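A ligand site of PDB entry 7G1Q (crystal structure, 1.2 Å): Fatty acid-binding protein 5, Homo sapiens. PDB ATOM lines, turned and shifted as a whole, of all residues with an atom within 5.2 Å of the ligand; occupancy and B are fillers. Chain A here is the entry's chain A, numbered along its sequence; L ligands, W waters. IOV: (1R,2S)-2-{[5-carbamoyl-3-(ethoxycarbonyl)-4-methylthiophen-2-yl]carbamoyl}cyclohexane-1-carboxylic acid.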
ATOM      1  N   PHE A  22      15.986 -22.115 -36.694  1.00  0.00           N
ATOM      2  CA  PHE A  22      15.491 -20.836 -36.175  1.00  0.00           C
ATOM      3  C   PHE A  22      16.370 -19.630 -36.541  1.00  0.00           C
ATOM      4  O   PHE A  22      15.895 -18.557 -36.809  1.00  0.00           O
ATOM      5  CB  PHE A  22      15.191 -20.939 -34.688  1.00  0.00           C
ATOM      6  CG  PHE A  22      14.368 -19.816 -34.147  1.00  0.00           C
ATOM      7  CD1 PHE A  22      13.127 -19.544 -34.650  1.00  0.00           C
ATOM      8  CD2 PHE A  22      14.831 -19.037 -33.086  1.00  0.00           C
ATOM      9  CE1 PHE A  22      12.350 -18.501 -34.154  1.00  0.00           C
ATOM     10  CE2 PHE A  22      14.056 -18.032 -32.551  1.00  0.00           C
ATOM     11  CZ  PHE A  22      12.898 -17.725 -33.105  1.00  0.00           C
ATOM     12  N   TYR A  25      15.594 -18.705 -40.016  1.00  0.00           N
ATOM     13  CA  TYR A  25      14.320 -18.047 -40.066  1.00  0.00           C
ATOM     14  C   TYR A  25      14.388 -16.578 -39.594  1.00  0.00           C
ATOM     15  O   TYR A  25      13.843 -15.705 -40.228  1.00  0.00           O
ATOM     16  CB  TYR A  25      13.277 -18.864 -39.235  1.00  0.00           C
ATOM     17  CG  TYR A  25      11.921 -18.255 -39.144  1.00  0.00           C
ATOM     18  CD1 TYR A  25      11.029 -18.253 -40.236  1.00  0.00           C
ATOM     19  CD2 TYR A  25      11.453 -17.698 -37.942  1.00  0.00           C
ATOM     20  CE1 TYR A  25       9.824 -17.733 -40.145  1.00  0.00           C
ATOM     21  CE2 TYR A  25      10.203 -17.194 -37.868  1.00  0.00           C
ATOM     22  CZ  TYR A  25       9.391 -17.182 -38.949  1.00  0.00           C
ATOM     23  OH  TYR A  25       8.131 -16.643 -38.847  1.00  0.00           O
ATOM     24  N   MET A  26      15.101 -16.347 -38.489  1.00  0.00           N
ATOM     25  CA  MET A  26      15.276 -14.958 -38.017  1.00  0.00           C
ATOM     26  C   MET A  26      16.034 -14.133 -39.038  1.00  0.00           C
ATOM     27  O   MET A  26      15.726 -12.939 -39.204  1.00  0.00           O
ATOM     28  CB  MET A  26      16.016 -14.933 -36.660  1.00  0.00           C
ATOM     29  CG  MET A  26      15.245 -15.492 -35.525  1.00  0.00           C
ATOM     30  SD  MET A  26      16.022 -15.183 -33.939  1.00  0.00           S
ATOM     31  CE  MET A  26      17.401 -16.369 -34.003  1.00  0.00           C
ATOM     32  N   VAL A  31      16.006  -9.931 -38.762  1.00  0.00           N
ATOM     33  CA  VAL A  31      16.228  -9.594 -37.346  1.00  0.00           C
ATOM     34  C   VAL A  31      17.703  -9.308 -37.181  1.00  0.00           C
ATOM     35  O   VAL A  31      18.582 -10.003 -37.724  1.00  0.00           O
ATOM     36  CB  VAL A  31      15.763 -10.818 -36.428  1.00  0.00           C
ATOM     37  CG1 VAL A  31      16.031 -10.536 -34.954  1.00  0.00           C
ATOM     38  CG2 VAL A  31      14.319 -11.152 -36.625  1.00  0.00           C
ATOM     39  N   LEU A  35      18.736  -9.220 -31.199  1.00  0.00           N
ATOM     40  CA  LEU A  35      17.598 -10.102 -31.110  1.00  0.00           C
ATOM     41  C   LEU A  35      17.883 -11.530 -31.633  1.00  0.00           C
ATOM     42  O   LEU A  35      17.340 -12.479 -31.081  1.00  0.00           O
ATOM     43  CB  LEU A  35      16.373  -9.504 -31.749  1.00  0.00           C
ATOM     44  CG  LEU A  35      15.681  -8.374 -30.969  1.00  0.00           C
ATOM     45  CD1 LEU A  35      14.786  -7.534 -31.899  1.00  0.00           C
ATOM     46  CD2 LEU A  35      14.941  -8.965 -29.802  1.00  0.00           C
ATOM     47  N   MET A  38      19.564 -13.312 -28.802  1.00  0.00           N
ATOM     48  CA  MET A  38      18.537 -13.704 -27.833  1.00  0.00           C
ATOM     49  C   MET A  38      17.770 -14.916 -28.360  1.00  0.00           C
ATOM     50  O   MET A  38      17.516 -15.840 -27.594  1.00  0.00           O
ATOM     51  CB  MET A  38      17.609 -12.536 -27.619  1.00  0.00           C
ATOM     52  CG  MET A  38      18.197 -11.399 -26.860  1.00  0.00           C
ATOM     53  SD  MET A  38      17.149  -9.935 -26.713  1.00  0.00           S
ATOM     54  CE  MET A  38      15.749 -10.811 -26.025  1.00  0.00           C
ATOM     55  N   GLY A  39      17.323 -14.891 -29.622  1.00  0.00           N
ATOM     56  CA  GLY A  39      16.574 -16.014 -30.162  1.00  0.00           C
ATOM     57  C   GLY A  39      17.333 -17.309 -30.186  1.00  0.00           C
ATOM     58  O   GLY A  39      16.752 -18.369 -29.992  1.00  0.00           O
ATOM     59  N   ALA A  42      17.898 -18.162 -26.007  1.00  0.00           N
ATOM     60  CA  ALA A  42      16.766 -18.378 -25.141  1.00  0.00           C
ATOM     61  C   ALA A  42      16.246 -19.792 -25.223  1.00  0.00           C
ATOM     62  O   ALA A  42      16.154 -20.401 -26.338  1.00  0.00           O
ATOM     63  CB  ALA A  42      15.619 -17.394 -25.524  1.00  0.00           C
ATOM     64  N   PRO A  44      12.828 -20.842 -24.158  1.00  0.00           N
ATOM     65  CA  PRO A  44      11.541 -20.448 -23.572  1.00  0.00           C
ATOM     66  C   PRO A  44      10.640 -21.610 -23.194  1.00  0.00           C
ATOM     67  O   PRO A  44      10.683 -22.694 -23.779  1.00  0.00           O
ATOM     68  CB  PRO A  44      10.928 -19.599 -24.709  1.00  0.00           C
ATOM     69  CG  PRO A  44      11.475 -20.243 -25.985  1.00  0.00           C
ATOM     70  CD  PRO A  44      12.895 -20.534 -25.588  1.00  0.00           C
ATOM     71  N   THR A  59       5.147 -16.434 -23.632  1.00  0.00           N
ATOM     72  CA  THR A  59       6.418 -17.110 -23.565  1.00  0.00           C
ATOM     73  C   THR A  59       7.255 -16.526 -22.446  1.00  0.00           C
ATOM     74  O   THR A  59       7.043 -15.348 -22.081  1.00  0.00           O
ATOM     75  CB  THR A  59       7.197 -17.018 -24.826  1.00  0.00           C
ATOM     76  OG1 THR A  59       7.762 -15.711 -24.996  1.00  0.00           O
ATOM     77  CG2 THR A  59       6.360 -17.404 -26.055  1.00  0.00           C
ATOM     78  N   GLU A  60       8.082 -17.333 -21.861  1.00  0.00           N
ATOM     79  CA  GLU A  60       8.939 -16.921 -20.709  1.00  0.00           C
ATOM     80  C   GLU A  60      10.253 -17.616 -20.811  1.00  0.00           C
ATOM     81  O   GLU A  60      10.337 -18.873 -20.881  1.00  0.00           O
ATOM     82  CB  GLU A  60       8.317 -17.369 -19.389  1.00  0.00           C
ATOM     83  CG  GLU A  60       7.033 -16.737 -19.041  1.00  0.00           C
ATOM     84  CD  GLU A  60       6.512 -17.195 -17.668  1.00  0.00           C
ATOM     85  OE1 GLU A  60       6.585 -18.398 -17.293  1.00  0.00           O
ATOM     86  OE2 GLU A  60       5.941 -16.330 -17.037  1.00  0.00           O
ATOM     87  N   SER A  61      11.327 -16.847 -20.803  1.00  0.00           N
ATOM     88  CA  SER A  61      12.650 -17.399 -20.744  1.00  0.00           C
ATOM     89  C   SER A  61      13.460 -16.559 -19.780  1.00  0.00           C
ATOM     90  O   SER A  61      13.009 -15.482 -19.305  1.00  0.00           O
ATOM     91  CB  SER A  61      13.340 -17.371 -22.072  1.00  0.00           C
ATOM     92  OG  SER A  61      13.736 -16.042 -22.447  1.00  0.00           O
ATOM     93  N   LEU A  63      15.618 -14.546 -20.648  1.00  0.00           N
ATOM     94  CA  LEU A  63      15.853 -13.345 -21.383  1.00  0.00           C
ATOM     95  C   LEU A  63      14.658 -12.439 -21.543  1.00  0.00           C
ATOM     96  O   LEU A  63      14.804 -11.237 -21.492  1.00  0.00           O
ATOM     97  CB  LEU A  63      16.555 -13.606 -22.738  1.00  0.00           C
ATOM     98  CG  LEU A  63      17.809 -14.393 -22.629  1.00  0.00           C
ATOM     99  CD1 LEU A  63      18.430 -14.577 -23.996  1.00  0.00           C
ATOM    100  CD2 LEU A  63      18.835 -13.815 -21.630  1.00  0.00           C
ATOM    101  N   LYS A  64      13.469 -13.007 -21.794  1.00  0.00           N
ATOM    102  CA  LYS A  64      12.289 -12.273 -22.277  1.00  0.00           C
ATOM    103  C   LYS A  64      11.014 -13.000 -21.949  1.00  0.00           C
ATOM    104  O   LYS A  64      10.994 -14.255 -21.993  1.00  0.00           O
ATOM    105  CB  LYS A  64      12.432 -12.246 -23.872  1.00  0.00           C
ATOM    106  CG  LYS A  64      11.536 -11.292 -24.618  1.00  0.00           C
ATOM    107  CD  LYS A  64      11.939 -11.096 -26.093  1.00  0.00           C
ATOM    108  CE  LYS A  64      10.908 -10.342 -26.899  1.00  0.00           C
ATOM    109  NZ  LYS A  64      10.833  -8.902 -26.550  1.00  0.00           N
ATOM    110  N   THR A  65       9.976 -12.248 -21.760  1.00  0.00           N
ATOM    111  CA  THR A  65       8.601 -12.710 -21.625  1.00  0.00           C
ATOM    112  C   THR A  65       7.802 -11.997 -22.703  1.00  0.00           C
ATOM    113  O   THR A  65       7.926 -10.761 -22.807  1.00  0.00           O
ATOM    114  CB  THR A  65       8.027 -12.462 -20.227  1.00  0.00           C
ATOM    115  OG1 THR A  65       8.745 -13.315 -19.304  1.00  0.00           O
ATOM    116  CG2 THR A  65       6.518 -12.731 -20.112  1.00  0.00           C
ATOM    117  N   THR A  66       6.923 -12.688 -23.451  1.00  0.00           N
ATOM    118  CA  THR A  66       6.034 -12.085 -24.398  1.00  0.00           C
ATOM    119  C   THR A  66       4.611 -12.635 -24.208  1.00  0.00           C
ATOM    120  O   THR A  66       4.423 -13.701 -23.563  1.00  0.00           O
ATOM    121  CB  THR A  66       6.399 -12.443 -25.872  1.00  0.00           C
ATOM    122  OG1 THR A  66       6.180 -13.868 -26.120  1.00  0.00           O
ATOM    123  CG2 THR A  66       7.842 -12.082 -26.150  1.00  0.00           C
ATOM    124  N   ALA A  81       7.933 -10.991 -31.229  1.00  0.00           N
ATOM    125  CA  ALA A  81       9.092 -10.990 -30.318  1.00  0.00           C
ATOM    126  C   ALA A  81      10.232 -10.169 -30.941  1.00  0.00           C
ATOM    127  O   ALA A  81      11.070  -9.668 -30.220  1.00  0.00           O
ATOM    128  CB  ALA A  81       9.497 -12.435 -29.992  1.00  0.00           C
ATOM    129  N   ASP A  82      10.307 -10.079 -32.273  1.00  0.00           N
ATOM    130  CA  ASP A  82      11.254  -9.272 -32.972  1.00  0.00           C
ATOM    131  C   ASP A  82      10.849  -7.867 -33.309  1.00  0.00           C
ATOM    132  O   ASP A  82      11.636  -7.126 -33.891  1.00  0.00           O
ATOM    133  CB  ASP A  82      11.766 -10.006 -34.223  1.00  0.00           C
ATOM    134  CG  ASP A  82      10.650 -10.256 -35.249  1.00  0.00           C
ATOM    135  OD1 ASP A  82       9.738 -10.992 -34.854  1.00  0.00           O
ATOM    136  OD2 ASP A  82      10.752  -9.815 -36.399  1.00  0.00           O
ATOM    137  N   ILE A 110       3.159 -19.768 -38.762  1.00  0.00           N
ATOM    138  CA  ILE A 110       3.618 -20.587 -37.643  1.00  0.00           C
ATOM    139  C   ILE A 110       2.497 -21.585 -37.330  1.00  0.00           C
ATOM    140  O   ILE A 110       1.382 -21.207 -37.099  1.00  0.00           O
ATOM    141  CB  ILE A 110       3.851 -19.774 -36.347  1.00  0.00           C
ATOM    142  CG1 ILE A 110       4.893 -18.689 -36.586  1.00  0.00           C
ATOM    143  CG2 ILE A 110       4.283 -20.678 -35.219  1.00  0.00           C
ATOM    144  CD1 ILE A 110       4.848 -17.545 -35.573  1.00  0.00           C
ATOM    145  N   ARG A 112       1.337 -25.040 -34.889  1.00  0.00           N
ATOM    146  CA  ARG A 112       1.572 -25.751 -33.664  1.00  0.00           C
ATOM    147  C   ARG A 112       0.656 -26.979 -33.631  1.00  0.00           C
ATOM    148  O   ARG A 112      -0.518 -26.829 -33.814  1.00  0.00           O
ATOM    149  CB  ARG A 112       1.286 -24.819 -32.456  1.00  0.00           C
ATOM    150  CG  ARG A 112       2.207 -23.611 -32.387  1.00  0.00           C
ATOM    151  CD  ARG A 112       1.898 -22.787 -31.198  1.00  0.00           C
ATOM    152  NE  ARG A 112       2.857 -21.717 -30.946  1.00  0.00           N
ATOM    153  CZ  ARG A 112       2.757 -20.538 -31.519  1.00  0.00           C
ATOM    154  NH1 ARG A 112       1.826 -20.220 -32.392  1.00  0.00           N
ATOM    155  NH2 ARG A 112       3.630 -19.559 -31.128  1.00  0.00           N
ATOM    156  N   VAL A 121       6.304 -27.015 -33.190  1.00  0.00           N
ATOM    157  CA  VAL A 121       6.121 -25.687 -33.732  1.00  0.00           C
ATOM    158  C   VAL A 121       6.933 -25.602 -35.024  1.00  0.00           C
ATOM    159  O   VAL A 121       8.133 -25.877 -35.037  1.00  0.00           O
ATOM    160  CB  VAL A 121       6.564 -24.647 -32.679  1.00  0.00           C
ATOM    161  CG1 VAL A 121       6.327 -23.213 -33.210  1.00  0.00           C
ATOM    162  CG2 VAL A 121       5.769 -24.899 -31.366  1.00  0.00           C
ATOM    163  N   CYS A 123       7.785 -23.027 -38.362  1.00  0.00           N
ATOM    164  CA  CYS A 123       7.784 -21.660 -38.910  1.00  0.00           C
ATOM    165  C   CYS A 123       8.153 -21.697 -40.363  1.00  0.00           C
ATOM    166  O   CYS A 123       8.983 -22.528 -40.760  1.00  0.00           O
ATOM    167  CB  CYS A 123       8.826 -20.774 -38.193  1.00  0.00           C
ATOM    168  SG  CYS A 123       8.359 -20.666 -36.480  1.00  0.00           S
ATOM    169  N   ARG A 132      10.645 -26.429 -34.027  1.00  0.00           N
ATOM    170  CA  ARG A 132      10.964 -26.304 -32.628  1.00  0.00           C
ATOM    171  C   ARG A 132      10.055 -27.258 -31.832  1.00  0.00           C
ATOM    172  O   ARG A 132       8.869 -27.290 -32.050  1.00  0.00           O
ATOM    173  CB  ARG A 132      10.820 -24.891 -32.149  1.00  0.00           C
ATOM    174  CG  ARG A 132      11.826 -23.980 -32.809  1.00  0.00           C
ATOM    175  CD  ARG A 132      11.582 -22.503 -32.731  1.00  0.00           C
ATOM    176  NE  ARG A 132      11.523 -21.890 -31.405  1.00  0.00           N
ATOM    177  CZ  ARG A 132      12.569 -21.417 -30.730  1.00  0.00           C
ATOM    178  NH1 ARG A 132      13.781 -21.720 -31.063  1.00  0.00           N
ATOM    179  NH2 ARG A 132      12.372 -20.632 -29.644  1.00  0.00           N
ATOM    180  N   TYR A 134       8.742 -28.835 -28.200  1.00  0.00           N
ATOM    181  CA  TYR A 134       8.535 -28.531 -26.818  1.00  0.00           C
ATOM    182  C   TYR A 134       7.912 -29.727 -26.073  1.00  0.00           C
ATOM    183  O   TYR A 134       7.079 -30.455 -26.642  1.00  0.00           O
ATOM    184  CB  TYR A 134       7.525 -27.366 -26.686  1.00  0.00           C
ATOM    185  CG  TYR A 134       7.969 -25.997 -27.188  1.00  0.00           C
ATOM    186  CD1 TYR A 134       8.037 -25.704 -28.527  1.00  0.00           C
ATOM    187  CD2 TYR A 134       8.326 -24.989 -26.309  1.00  0.00           C
ATOM    188  CE1 TYR A 134       8.462 -24.441 -28.974  1.00  0.00           C
ATOM    189  CE2 TYR A 134       8.731 -23.736 -26.747  1.00  0.00           C
ATOM    190  CZ  TYR A 134       8.785 -23.473 -28.032  1.00  0.00           C
ATOM    191  OH  TYR A 134       9.208 -22.227 -28.462  1.00  0.00           O
HETATM  192  C1  IOV L   1      10.623 -16.082 -28.976  1.00  0.00           C
HETATM  193  C2  IOV L   1      11.848 -15.369 -28.994  1.00  0.00           C
HETATM  194  C3  IOV L   1      12.363 -15.159 -27.698  1.00  0.00           C
HETATM  195  C4  IOV L   1      11.500 -15.665 -26.728  1.00  0.00           C
HETATM  196  S5  IOV L   1      10.131 -16.403 -27.385  1.00  0.00           S
HETATM  197  N6  IOV L   1       9.897 -16.456 -30.128  1.00  0.00           N
HETATM  198  C7  IOV L   1       8.746 -17.193 -30.064  1.00  0.00           C
HETATM  199  C8  IOV L   1      12.432 -14.884 -30.194  1.00  0.00           C
HETATM  200  C9  IOV L   1      11.625 -15.649 -25.279  1.00  0.00           C
HETATM  201  C10 IOV L   1       8.147 -17.654 -31.347  1.00  0.00           C
HETATM  202  C11 IOV L   1       7.590 -19.069 -31.214  1.00  0.00           C
HETATM  203  C12 IOV L   1       8.602 -20.028 -30.711  1.00  0.00           C
HETATM  204  O13 IOV L   1       8.196 -17.447 -28.993  1.00  0.00           O
HETATM  205  O14 IOV L   1      13.494 -14.210 -30.219  1.00  0.00           O
HETATM  206  CA  IOV L   1      14.054 -13.625 -31.381  1.00  0.00           C
HETATM  207  CB  IOV L   1      13.364 -12.346 -31.793  1.00  0.00           C
HETATM  208  N15 IOV L   1      10.659 -15.668 -24.477  1.00  0.00           N
HETATM  209  O16 IOV L   1       8.481 -21.248 -30.731  1.00  0.00           O
HETATM  210  O17 IOV L   1      11.823 -15.070 -31.335  1.00  0.00           O
HETATM  211  C18 IOV L   1      13.639 -14.411 -27.478  1.00  0.00           C
HETATM  212  O19 IOV L   1       9.770 -19.589 -30.320  1.00  0.00           O
HETATM  213  O20 IOV L   1      12.843 -15.606 -24.806  1.00  0.00           O
HETATM  214  C21 IOV L   1       9.073 -17.469 -32.513  1.00  0.00           C
HETATM  215  C22 IOV L   1       6.970 -19.566 -32.507  1.00  0.00           C
HETATM  216  C24 IOV L   1       8.393 -17.941 -33.832  1.00  0.00           C
HETATM  217  C25 IOV L   1       7.895 -19.373 -33.718  1.00  0.00           C
HETATM  218  O   HOH W   1       7.009 -14.833 -28.778  1.00  0.00           O
HETATM  219  O   HOH W   2       5.560 -21.784 -29.742  1.00  0.00           O
HETATM  220  O   HOH W   3       7.884 -19.964 -27.409  1.00  0.00           O
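The side-chain hydroxyl of Thr 59 is in hydrogen-bond range of a nitrogen (N15) of the ligand, at 2.9 Å.
OG of Ser 61 lies within hydrogen-bond range of O20 of the ligand (2.6 Å).
The guanidinium group (NH2) of Arg 132 lies within salt-bridge range of an oxygen (O19) of the ligand (2.9 Å).
The backbone carbonyl oxygen (O) of Lys 64 lies within hydrogen-bond range of a nitrogen (N15) of the ligand.
The side-chain hydroxyl (OH) of Tyr 134 sits at hydrogen-bond distance from an oxygen (O16) of the ligand (2.6 Å).
The backbone NH (N) of Arg 132 sits at hydrogen-bond distance from the backbone carbonyl oxygen (O) of Val 121 (2.8 Å).
The backbone NH of Leu 63 lies within hydrogen-bond range of the side-chain hydroxyl of Ser 61, 3.0 Å away.
The side-chain hydroxyl (OG) of Ser 61 is in hydrogen-bond range of the backbone NH (N) of Lys 64 (3.1 Å).
The backbone carbonyl oxygen of Met 26 sits at hydrogen-bond distance from the backbone NH of Val 31, at 3.1 Å.
OG1 of Thr 59 is in hydrogen-bond range of OG1 of Thr 66 (2.7 Å).
CZ of Phe 22 touches O17 of the ligand, at 3.4 Å.
Met 26 touches the ligand (SD to CA, 3.6 Å).
Leu 35 touches the ligand.
Gly 39 touches the ligand.
Ala 42 touches the ligand.
Pro 44 touches the ligand (CB to N15, 3.9 Å).
Ala 81 touches the ligand (CB to O17, 3.8 Å).
CB of Asp 82 touches CB of the ligand, at 3.7 Å.
Ile 110 touches the ligand (CD1 to C24, 3.97 Å).
Arg 112 touches the ligand (NH2 to C22, 3.6 Å).
Val 121 touches the ligand (CG1 to C22, 3.8 Å).
SG of Cys 123 touches C25 of the ligand, 3.1 Å away.
Water W1 lies within hydrogen-bond range of O13 of the ligand (2.9 Å) and OG1 of Thr 66 (2.9 Å).
Water W3 bridges OH of Tyr 134 (2.8 Å) and O13 of the ligand (3.0 Å).
Water W2 lies within hydrogen-bond range of the guanidinium group of Arg 112 (3.0 Å) and an oxygen (O16) of the ligand (3.1 Å).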
